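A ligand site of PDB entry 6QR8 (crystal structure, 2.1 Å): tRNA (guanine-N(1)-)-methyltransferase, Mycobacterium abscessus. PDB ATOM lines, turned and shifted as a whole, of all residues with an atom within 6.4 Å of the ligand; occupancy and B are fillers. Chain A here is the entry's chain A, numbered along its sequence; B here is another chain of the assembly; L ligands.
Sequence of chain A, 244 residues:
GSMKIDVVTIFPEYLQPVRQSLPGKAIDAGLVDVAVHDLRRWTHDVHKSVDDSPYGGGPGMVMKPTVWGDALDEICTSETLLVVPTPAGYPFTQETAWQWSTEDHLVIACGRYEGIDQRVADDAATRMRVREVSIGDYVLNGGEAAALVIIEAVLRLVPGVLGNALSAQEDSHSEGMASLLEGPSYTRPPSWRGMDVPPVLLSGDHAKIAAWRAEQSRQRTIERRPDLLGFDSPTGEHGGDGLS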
ATOM      1  N   VAL A  84       6.042  27.023 -34.190  1.00  0.00           N
ATOM      2  CA  VAL A  84       6.546  27.868 -33.114  1.00  0.00           C
ATOM      3  C   VAL A  84       6.623  27.090 -31.790  1.00  0.00           C
ATOM      4  O   VAL A  84       5.610  26.878 -31.111  1.00  0.00           O
ATOM      5  CB  VAL A  84       5.663  29.121 -32.898  1.00  0.00           C
ATOM      6  CG1 VAL A  84       6.282  30.019 -31.841  1.00  0.00           C
ATOM      7  CG2 VAL A  84       5.474  29.898 -34.227  1.00  0.00           C
ATOM      8  N   PRO A  85       7.830  26.642 -31.417  1.00  0.00           N
ATOM      9  CA  PRO A  85       7.986  25.990 -30.113  1.00  0.00           C
ATOM     10  C   PRO A  85       7.605  26.959 -29.009  1.00  0.00           C
ATOM     11  O   PRO A  85       7.897  28.147 -29.124  1.00  0.00           O
ATOM     12  CB  PRO A  85       9.485  25.667 -30.064  1.00  0.00           C
ATOM     13  CG  PRO A  85       9.902  25.623 -31.495  1.00  0.00           C
ATOM     14  CD  PRO A  85       9.111  26.721 -32.142  1.00  0.00           C
ATOM     15  N   THR A  86       6.941  26.457 -27.973  1.00  0.00           N
ATOM     16  CA  THR A  86       6.562  27.289 -26.840  1.00  0.00           C
ATOM     17  C   THR A  86       6.136  26.393 -25.692  1.00  0.00           C
ATOM     18  O   THR A  86       5.528  25.347 -25.905  1.00  0.00           O
ATOM     19  CB  THR A  86       5.410  28.292 -27.178  1.00  0.00           C
ATOM     20  OG1 THR A  86       4.781  28.754 -25.968  1.00  0.00           O
ATOM     21  CG2 THR A  86       4.354  27.680 -28.085  1.00  0.00           C
ATOM     22  N   PRO A  87       6.467  26.793 -24.463  1.00  0.00           N
ATOM     23  CA  PRO A  87       6.073  25.995 -23.296  1.00  0.00           C
ATOM     24  C   PRO A  87       4.555  25.966 -23.155  1.00  0.00           C
ATOM     25  O   PRO A  87       4.036  25.168 -22.400  1.00  0.00           O
ATOM     26  CB  PRO A  87       6.743  26.705 -22.106  1.00  0.00           C
ATOM     27  CG  PRO A  87       7.051  28.080 -22.599  1.00  0.00           C
ATOM     28  CD  PRO A  87       7.183  28.029 -24.096  1.00  0.00           C
ATOM     29  N   ALA A  88       3.851  26.804 -23.900  1.00  0.00           N
ATOM     30  CA  ALA A  88       2.408  26.828 -23.794  1.00  0.00           C
ATOM     31  C   ALA A  88       1.731  26.249 -25.019  1.00  0.00           C
ATOM     32  O   ALA A  88       0.548  26.502 -25.250  1.00  0.00           O
ATOM     33  CB  ALA A  88       1.925  28.234 -23.542  1.00  0.00           C
ATOM     34  N   CYS A 110      12.389  30.018 -33.482  1.00  0.00           N
ATOM     35  CA  CYS A 110      12.908  29.779 -32.139  1.00  0.00           C
ATOM     36  C   CYS A 110      12.976  31.030 -31.273  1.00  0.00           C
ATOM     37  O   CYS A 110      13.784  31.922 -31.529  1.00  0.00           O
ATOM     38  CB  CYS A 110      14.298  29.163 -32.212  1.00  0.00           C
ATOM     39  SG  CYS A 110      14.361  27.624 -33.113  1.00  0.00           S
ATOM     40  N   GLY A 111      12.183  31.069 -30.219  1.00  0.00           N
ATOM     41  CA  GLY A 111      12.212  32.210 -29.315  1.00  0.00           C
ATOM     42  C   GLY A 111      13.216  32.060 -28.192  1.00  0.00           C
ATOM     43  O   GLY A 111      13.831  30.987 -27.997  1.00  0.00           O
ATOM     44  N   ARG A 112      13.395  33.155 -27.473  1.00  0.00           N
ATOM     45  CA  ARG A 112      14.193  33.215 -26.248  1.00  0.00           C
ATOM     46  C   ARG A 112      13.446  34.112 -25.277  1.00  0.00           C
ATOM     47  O   ARG A 112      12.340  34.543 -25.581  1.00  0.00           O
ATOM     48  CB  ARG A 112      15.588  33.765 -26.517  1.00  0.00           C
ATOM     49  CG  ARG A 112      16.514  32.774 -27.157  1.00  0.00           C
ATOM     50  CD  ARG A 112      17.294  32.026 -26.106  1.00  0.00           C
ATOM     51  NE  ARG A 112      17.573  30.672 -26.566  1.00  0.00           N
ATOM     52  CZ  ARG A 112      18.271  29.786 -25.869  1.00  0.00           C
ATOM     53  NH1 ARG A 112      18.752  30.114 -24.678  1.00  0.00           N
ATOM     54  NH2 ARG A 112      18.473  28.567 -26.362  1.00  0.00           N
ATOM     55  N   TYR A 113      14.059  34.396 -24.131  1.00  0.00           N
ATOM     56  CA  TYR A 113      13.438  35.226 -23.099  1.00  0.00           C
ATOM     57  C   TYR A 113      12.083  34.632 -22.740  1.00  0.00           C
ATOM     58  O   TYR A 113      11.974  33.426 -22.568  1.00  0.00           O
ATOM     59  CB  TYR A 113      13.296  36.684 -23.568  1.00  0.00           C
ATOM     60  CG  TYR A 113      14.588  37.228 -24.132  1.00  0.00           C
ATOM     61  CD1 TYR A 113      15.619  37.619 -23.287  1.00  0.00           C
ATOM     62  CD2 TYR A 113      14.793  37.323 -25.503  1.00  0.00           C
ATOM     63  CE1 TYR A 113      16.815  38.107 -23.785  1.00  0.00           C
ATOM     64  CE2 TYR A 113      15.987  37.812 -26.015  1.00  0.00           C
ATOM     65  CZ  TYR A 113      16.996  38.201 -25.153  1.00  0.00           C
ATOM     66  OH  TYR A 113      18.192  38.689 -25.651  1.00  0.00           O
ATOM     67  N   GLU A 114      11.046  35.455 -22.668  1.00  0.00           N
ATOM     68  CA  GLU A 114       9.716  34.955 -22.309  1.00  0.00           C
ATOM     69  C   GLU A 114       8.923  34.511 -23.525  1.00  0.00           C
ATOM     70  O   GLU A 114       7.769  34.134 -23.395  1.00  0.00           O
ATOM     71  CB  GLU A 114       8.929  36.006 -21.540  1.00  0.00           C
ATOM     72  CG  GLU A 114       9.620  36.440 -20.260  1.00  0.00           C
ATOM     73  CD  GLU A 114       9.944  35.267 -19.358  1.00  0.00           C
ATOM     74  OE1 GLU A 114       8.993  34.685 -18.790  1.00  0.00           O
ATOM     75  OE2 GLU A 114      11.140  34.904 -19.240  1.00  0.00           O
ATOM     76  N   GLY A 115       9.543  34.561 -24.695  1.00  0.00           N
ATOM     77  CA  GLY A 115       8.866  34.185 -25.913  1.00  0.00           C
ATOM     78  C   GLY A 115       8.621  35.375 -26.840  1.00  0.00           C
ATOM     79  O   GLY A 115       9.179  36.445 -26.653  1.00  0.00           O
ATOM     80  N   ILE A 116       7.752  35.165 -27.819  1.00  0.00           N
ATOM     81  CA  ILE A 116       7.551  36.108 -28.920  1.00  0.00           C
ATOM     82  C   ILE A 116       6.229  36.838 -28.766  1.00  0.00           C
ATOM     83  O   ILE A 116       5.236  36.227 -28.418  1.00  0.00           O
ATOM     84  CB  ILE A 116       7.583  35.336 -30.269  1.00  0.00           C
ATOM     85  CG1 ILE A 116       8.871  34.526 -30.397  1.00  0.00           C
ATOM     86  CG2 ILE A 116       7.408  36.262 -31.477  1.00  0.00           C
ATOM     87  CD1 ILE A 116       9.017  33.797 -31.744  1.00  0.00           C
ATOM     88  N   VAL A 133       3.602  24.504 -30.573  1.00  0.00           N
ATOM     89  CA  VAL A 133       3.713  23.193 -29.963  1.00  0.00           C
ATOM     90  C   VAL A 133       4.749  23.173 -28.859  1.00  0.00           C
ATOM     91  O   VAL A 133       5.669  23.999 -28.844  1.00  0.00           O
ATOM     92  CB  VAL A 133       4.093  22.088 -30.994  1.00  0.00           C
ATOM     93  CG1 VAL A 133       2.983  21.919 -32.034  1.00  0.00           C
ATOM     94  CG2 VAL A 133       5.416  22.418 -31.664  1.00  0.00           C
ATOM     95  N   SER A 134       4.590  22.222 -27.943  1.00  0.00           N
ATOM     96  CA  SER A 134       5.561  21.984 -26.874  1.00  0.00           C
ATOM     97  C   SER A 134       6.111  20.560 -26.986  1.00  0.00           C
ATOM     98  O   SER A 134       5.347  19.625 -27.244  1.00  0.00           O
ATOM     99  CB  SER A 134       4.908  22.192 -25.514  1.00  0.00           C
ATOM    100  OG  SER A 134       5.776  21.709 -24.520  1.00  0.00           O
ATOM    101  N   ILE A 135       7.417  20.378 -26.794  1.00  0.00           N
ATOM    102  CA  ILE A 135       7.962  19.016 -26.892  1.00  0.00           C
ATOM    103  C   ILE A 135       7.865  18.182 -25.592  1.00  0.00           C
ATOM    104  O   ILE A 135       8.249  17.017 -25.567  1.00  0.00           O
ATOM    105  CB  ILE A 135       9.448  19.026 -27.353  1.00  0.00           C
ATOM    106  CG1 ILE A 135      10.336  19.781 -26.363  1.00  0.00           C
ATOM    107  CG2 ILE A 135       9.586  19.588 -28.766  1.00  0.00           C
ATOM    108  CD1 ILE A 135      11.804  19.445 -26.527  1.00  0.00           C
ATOM    109  N   GLY A 136       7.358  18.761 -24.510  1.00  0.00           N
ATOM    110  CA  GLY A 136       7.241  18.042 -23.252  1.00  0.00           C
ATOM    111  C   GLY A 136       7.024  18.954 -22.063  1.00  0.00           C
ATOM    112  O   GLY A 136       7.090  20.188 -22.182  1.00  0.00           O
ATOM    113  N   ASP A 137       6.765  18.363 -20.901  1.00  0.00           N
ATOM    114  CA  ASP A 137       6.296  19.127 -19.755  1.00  0.00           C
ATOM    115  C   ASP A 137       7.431  19.527 -18.845  1.00  0.00           C
ATOM    116  O   ASP A 137       7.493  19.098 -17.699  1.00  0.00           O
ATOM    117  CB  ASP A 137       5.235  18.346 -18.976  1.00  0.00           C
ATOM    118  CG  ASP A 137       3.870  18.392 -19.655  1.00  0.00           C
ATOM    119  OD1 ASP A 137       3.565  19.408 -20.324  1.00  0.00           O
ATOM    120  OD2 ASP A 137       3.093  17.420 -19.519  1.00  0.00           O
ATOM    121  N   TYR A 138       8.357  20.319 -19.381  1.00  0.00           N
ATOM    122  CA  TYR A 138       9.501  20.806 -18.643  1.00  0.00           C
ATOM    123  C   TYR A 138       9.784  22.147 -19.265  1.00  0.00           C
ATOM    124  O   TYR A 138       9.202  22.468 -20.296  1.00  0.00           O
ATOM    125  CB  TYR A 138      10.714  19.877 -18.758  1.00  0.00           C
ATOM    126  CG  TYR A 138      10.805  19.235 -20.116  1.00  0.00           C
ATOM    127  CD1 TYR A 138      11.299  19.942 -21.215  1.00  0.00           C
ATOM    128  CD2 TYR A 138      10.368  17.925 -20.310  1.00  0.00           C
ATOM    129  CE1 TYR A 138      11.361  19.369 -22.461  1.00  0.00           C
ATOM    130  CE2 TYR A 138      10.424  17.338 -21.542  1.00  0.00           C
ATOM    131  CZ  TYR A 138      10.922  18.059 -22.611  1.00  0.00           C
ATOM    132  OH  TYR A 138      10.953  17.448 -23.835  1.00  0.00           O
ATOM    133  N   VAL A 139      10.644  22.949 -18.661  1.00  0.00           N
ATOM    134  CA  VAL A 139      10.865  24.312 -19.128  1.00  0.00           C
ATOM    135  C   VAL A 139      12.279  24.420 -19.654  1.00  0.00           C
ATOM    136  O   VAL A 139      13.214  24.014 -18.978  1.00  0.00           O
ATOM    137  CB  VAL A 139      10.650  25.341 -17.999  1.00  0.00           C
ATOM    138  CG1 VAL A 139      10.936  26.756 -18.491  1.00  0.00           C
ATOM    139  CG2 VAL A 139       9.245  25.236 -17.438  1.00  0.00           C
ATOM    140  N   LEU A 140      12.422  24.944 -20.871  1.00  0.00           N
ATOM    141  CA  LEU A 140      13.748  25.145 -21.476  1.00  0.00           C
ATOM    142  C   LEU A 140      14.096  26.641 -21.473  1.00  0.00           C
ATOM    143  O   LEU A 140      13.287  27.465 -21.076  1.00  0.00           O
ATOM    144  CB  LEU A 140      13.749  24.571 -22.893  1.00  0.00           C
ATOM    145  CG  LEU A 140      13.326  23.090 -23.012  1.00  0.00           C
ATOM    146  CD1 LEU A 140      13.124  22.683 -24.468  1.00  0.00           C
ATOM    147  CD2 LEU A 140      14.335  22.179 -22.370  1.00  0.00           C
ATOM    148  N   ASN A 141      15.288  27.005 -21.948  1.00  0.00           N
ATOM    149  CA  ASN A 141      15.685  28.420 -22.090  1.00  0.00           C
ATOM    150  C   ASN A 141      15.146  29.120 -23.347  1.00  0.00           C
ATOM    151  O   ASN A 141      15.115  30.358 -23.416  1.00  0.00           O
ATOM    152  CB  ASN A 141      17.198  28.552 -22.118  1.00  0.00           C
ATOM    153  CG  ASN A 141      17.833  28.305 -20.778  1.00  0.00           C
ATOM    154  OD1 ASN A 141      17.302  28.713 -19.739  1.00  0.00           O
ATOM    155  ND2 ASN A 141      18.954  27.603 -20.771  1.00  0.00           N
ATOM    156  N   GLY A 142      14.759  28.332 -24.334  1.00  0.00           N
ATOM    157  CA  GLY A 142      14.405  28.886 -25.640  1.00  0.00           C
ATOM    158  C   GLY A 142      13.994  27.784 -26.577  1.00  0.00           C
ATOM    159  O   GLY A 142      14.038  26.612 -26.194  1.00  0.00           O
ATOM    160  N   GLY A 143      13.615  28.126 -27.808  1.00  0.00           N
ATOM    161  CA  GLY A 143      13.063  27.158 -28.732  1.00  0.00           C
ATOM    162  C   GLY A 143      14.063  26.246 -29.440  1.00  0.00           C
ATOM    163  O   GLY A 143      13.673  25.289 -30.099  1.00  0.00           O
ATOM    164  N   GLU A 144      15.353  26.540 -29.304  1.00  0.00           N
ATOM    165  CA  GLU A 144      16.366  25.840 -30.092  1.00  0.00           C
ATOM    166  C   GLU A 144      16.451  24.319 -29.808  1.00  0.00           C
ATOM    167  O   GLU A 144      16.451  23.515 -30.753  1.00  0.00           O
ATOM    168  CB  GLU A 144      17.743  26.508 -29.894  1.00  0.00           C
ATOM    169  CG  GLU A 144      17.862  27.898 -30.580  1.00  0.00           C
ATOM    170  CD  GLU A 144      17.260  29.065 -29.754  1.00  0.00           C
ATOM    171  OE1 GLU A 144      16.780  28.830 -28.616  1.00  0.00           O
ATOM    172  OE2 GLU A 144      17.255  30.222 -30.251  1.00  0.00           O
ATOM    173  N   ALA A 146      14.133  22.466 -28.683  1.00  0.00           N
ATOM    174  CA  ALA A 146      12.877  21.898 -29.182  1.00  0.00           C
ATOM    175  C   ALA A 146      12.948  21.735 -30.682  1.00  0.00           C
ATOM    176  O   ALA A 146      12.394  20.792 -31.237  1.00  0.00           O
ATOM    177  CB  ALA A 146      11.688  22.776 -28.803  1.00  0.00           C
ATOM    178  N   ILE A 150      12.232  18.312 -32.755  1.00  0.00           N
ATOM    179  CA  ILE A 150      11.209  18.314 -33.797  1.00  0.00           C
ATOM    180  C   ILE A 150      11.787  17.937 -35.164  1.00  0.00           C
ATOM    181  O   ILE A 150      11.206  17.139 -35.894  1.00  0.00           O
ATOM    182  CB  ILE A 150      10.527  19.701 -33.906  1.00  0.00           C
ATOM    183  CG1 ILE A 150       9.628  19.952 -32.693  1.00  0.00           C
ATOM    184  CG2 ILE A 150       9.701  19.803 -35.190  1.00  0.00           C
ATOM    185  CD1 ILE A 150       9.063  21.353 -32.638  1.00  0.00           C
ATOM    186  N   ARG B 156      19.258  25.010 -15.788  1.00  0.00           N
ATOM    187  CA  ARG B 156      18.690  26.319 -15.520  1.00  0.00           C
ATOM    188  C   ARG B 156      18.046  26.401 -14.131  1.00  0.00           C
ATOM    189  O   ARG B 156      17.639  27.477 -13.702  1.00  0.00           O
ATOM    190  CB  ARG B 156      17.682  26.717 -16.624  1.00  0.00           C
ATOM    191  CG  ARG B 156      16.518  25.790 -16.794  1.00  0.00           C
ATOM    192  CD  ARG B 156      15.691  26.172 -18.027  1.00  0.00           C
ATOM    193  NE  ARG B 156      15.040  27.477 -17.912  1.00  0.00           N
ATOM    194  CZ  ARG B 156      14.081  27.770 -17.044  1.00  0.00           C
ATOM    195  NH1 ARG B 156      13.650  26.862 -16.170  1.00  0.00           N
ATOM    196  NH2 ARG B 156      13.547  28.973 -17.036  1.00  0.00           N
ATOM    197  N   ALA B 178       2.241  26.946 -11.768  1.00  0.00           N
ATOM    198  CA  ALA B 178       1.700  25.882 -10.929  1.00  0.00           C
ATOM    199  C   ALA B 178       1.594  24.579 -11.701  1.00  0.00           C
ATOM    200  O   ALA B 178       2.350  23.626 -11.494  1.00  0.00           O
ATOM    201  CB  ALA B 178       0.321  26.283 -10.377  1.00  0.00           C
ATOM    202  N   LEU B 180      -0.195  25.150 -15.116  1.00  0.00           N
ATOM    203  CA  LEU B 180      -1.000  25.871 -16.088  1.00  0.00           C
ATOM    204  C   LEU B 180      -0.135  26.428 -17.206  1.00  0.00           C
ATOM    205  O   LEU B 180       1.064  26.621 -17.016  1.00  0.00           O
ATOM    206  CB  LEU B 180      -1.760  27.015 -15.420  1.00  0.00           C
ATOM    207  CG  LEU B 180      -2.890  26.642 -14.453  1.00  0.00           C
ATOM    208  CD1 LEU B 180      -3.421  27.906 -13.821  1.00  0.00           C
ATOM    209  CD2 LEU B 180      -3.988  25.887 -15.181  1.00  0.00           C
ATOM    210  N   LEU B 181      -0.735  26.686 -18.363  1.00  0.00           N
ATOM    211  CA  LEU B 181      -0.010  27.224 -19.512  1.00  0.00           C
ATOM    212  C   LEU B 181      -0.026  28.740 -19.512  1.00  0.00           C
ATOM    213  O   LEU B 181      -1.085  29.340 -19.374  1.00  0.00           O
ATOM    214  CB  LEU B 181      -0.626  26.725 -20.810  1.00  0.00           C
ATOM    215  CG  LEU B 181      -0.685  25.226 -21.042  1.00  0.00           C
ATOM    216  CD1 LEU B 181      -1.064  24.952 -22.487  1.00  0.00           C
ATOM    217  CD2 LEU B 181       0.650  24.585 -20.671  1.00  0.00           C
ATOM    218  N   GLU B 182       1.137  29.348 -19.677  1.00  0.00           N
ATOM    219  CA  GLU B 182       1.233  30.799 -19.750  1.00  0.00           C
ATOM    220  C   GLU B 182       0.423  31.355 -20.924  1.00  0.00           C
ATOM    221  O   GLU B 182       0.484  30.825 -22.029  1.00  0.00           O
ATOM    222  CB  GLU B 182       2.699  31.226 -19.877  1.00  0.00           C
HETATM  223  C1  LIG L   1      10.308  28.205 -26.655  1.00  0.00           C
HETATM  224  C2  LIG L   1      11.550  31.098 -24.699  1.00  0.00           C
HETATM  225  C3  LIG L   1      11.842  30.155 -22.433  1.00  0.00           C
HETATM  226  C4  LIG L   1       9.496  31.047 -21.998  1.00  0.00           C
HETATM  227  C5  LIG L   1       7.236  31.255 -18.843  1.00  0.00           C
HETATM  228  C6  LIG L   1       6.676  29.152 -18.777  1.00  0.00           C
HETATM  229  C7  LIG L   1       5.424  29.440 -16.373  1.00  0.00           C
HETATM  230  C8  LIG L   1       9.655  30.306 -19.274  1.00  0.00           C
HETATM  231  N1  LIG L   1       8.635  21.892 -23.799  1.00  0.00           N
HETATM  232  C9  LIG L   1       9.208  23.206 -23.661  1.00  0.00           C
HETATM  233  N2  LIG L   1       9.689  23.771 -22.517  1.00  0.00           N
HETATM  234  N3  LIG L   1      10.144  25.014 -22.829  1.00  0.00           N
HETATM  235  C10 LIG L   1      10.036  25.246 -24.154  1.00  0.00           C
HETATM  236  C11 LIG L   1      10.363  26.609 -24.809  1.00  0.00           C
HETATM  237  C12 LIG L   1      10.791  27.633 -23.954  1.00  0.00           C
HETATM  238  C13 LIG L   1      11.023  28.948 -24.449  1.00  0.00           C
HETATM  239  C14 LIG L   1      10.786  29.230 -25.793  1.00  0.00           C
HETATM  240  C15 LIG L   1      10.079  26.898 -26.167  1.00  0.00           C
HETATM  241  C16 LIG L   1      11.126  30.615 -25.944  1.00  0.00           C
HETATM  242  N4  LIG L   1      11.483  30.079 -23.825  1.00  0.00           N
HETATM  243  C17 LIG L   1      10.657  30.418 -21.514  1.00  0.00           C
HETATM  244  C18 LIG L   1       8.421  31.306 -21.124  1.00  0.00           C
HETATM  245  C19 LIG L   1       8.479  30.937 -19.777  1.00  0.00           C
HETATM  246  N5  LIG L   1       6.937  30.261 -18.054  1.00  0.00           N
HETATM  247  C20 LIG L   1       6.316  27.962 -17.899  1.00  0.00           C
HETATM  248  N6  LIG L   1       5.365  28.223 -16.957  1.00  0.00           N
HETATM  249  C21 LIG L   1       4.185  27.926 -17.368  1.00  0.00           C
HETATM  250  C22 LIG L   1       5.857  30.584 -17.281  1.00  0.00           C
HETATM  251  C23 LIG L   1      10.734  30.053 -20.155  1.00  0.00           C
HETATM  252  C24 LIG L   1       9.403  24.143 -24.707  1.00  0.00           C
HETATM  253  C25 LIG L   1       9.015  23.866 -26.130  1.00  0.00           C
HETATM  254  N7  LIG L   1       8.708  23.610 -27.181  1.00  0.00           N
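The backbone carbonyl oxygen (O) of Ile 135 lies within hydrogen-bond range of the side-chain hydroxyl (OH) of Tyr 138, at 3.2 Å. O of Gly 136 lies within hydrogen-bond range of OG of Ser 134, at 3.1 Å. The backbone carbonyl oxygen of Gly 111 sits at hydrogen-bond distance from the backbone NH of Gly 143, at 2.9 Å. OD1 of Asn 141 sits at hydrogen-bond distance from NE of Arg 156 of chain B (3.2 Å). The backbone NH (N) of Thr 86 lies within hydrogen-bond range of the backbone carbonyl oxygen (O) of Val 133. N of Ala 88 lies close to OG1 of Thr 86, at 3.0 Å. The backbone carbonyl oxygen (O) of Val 84 is in hydrogen-bond range of the backbone NH (N) of Val 133, 3.2 Å away. NH2 of Arg 112 lies within salt-bridge range of OE1 of Glu 144 (2.8 Å).
O of Tyr 138 sits at hydrogen-bond distance from N2 of the ligand. The backbone carbonyl oxygen (O) of Gly 136 sits at hydrogen-bond distance from a nitrogen (N1) of the ligand (2.8 Å). OG of Ser 134 sits at hydrogen-bond distance from N1 of the ligand. A nitrogen (N3) of the ligand sits at hydrogen-bond distance from the backbone NH (N) of Leu 140 (3.0 Å). N of Thr 86 is in hydrogen-bond range of N7 of the ligand, at 3.4 Å.
The backbone carbonyl oxygen (O) of Val 133 sits close to a nitrogen (N7) of the ligand (3.5 Å). O of Pro 85 touches C1 of the ligand, 3.5 Å away. CD of Pro 87 touches C11 of the ligand, at 3.6 Å. Gly 111 touches the ligand. Arg 112 touches the ligand. Tyr 113 touches the ligand (O to C2, 3.2 Å). O of Glu 114 touches C18 of the ligand, at 3.7 Å. Ile 135 touches the ligand. Val 139 touches the ligand. Asn 141 touches the ligand. CA of Gly 142 touches C13 of the ligand, at 3.6 Å. Gly 143 touches the ligand. Ala 146 touches the ligand (CB to N7, 3.5 Å). Leu 180 of chain B touches the ligand. Of the 31 residues printed, 19 come within 4 Å of the ligand.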
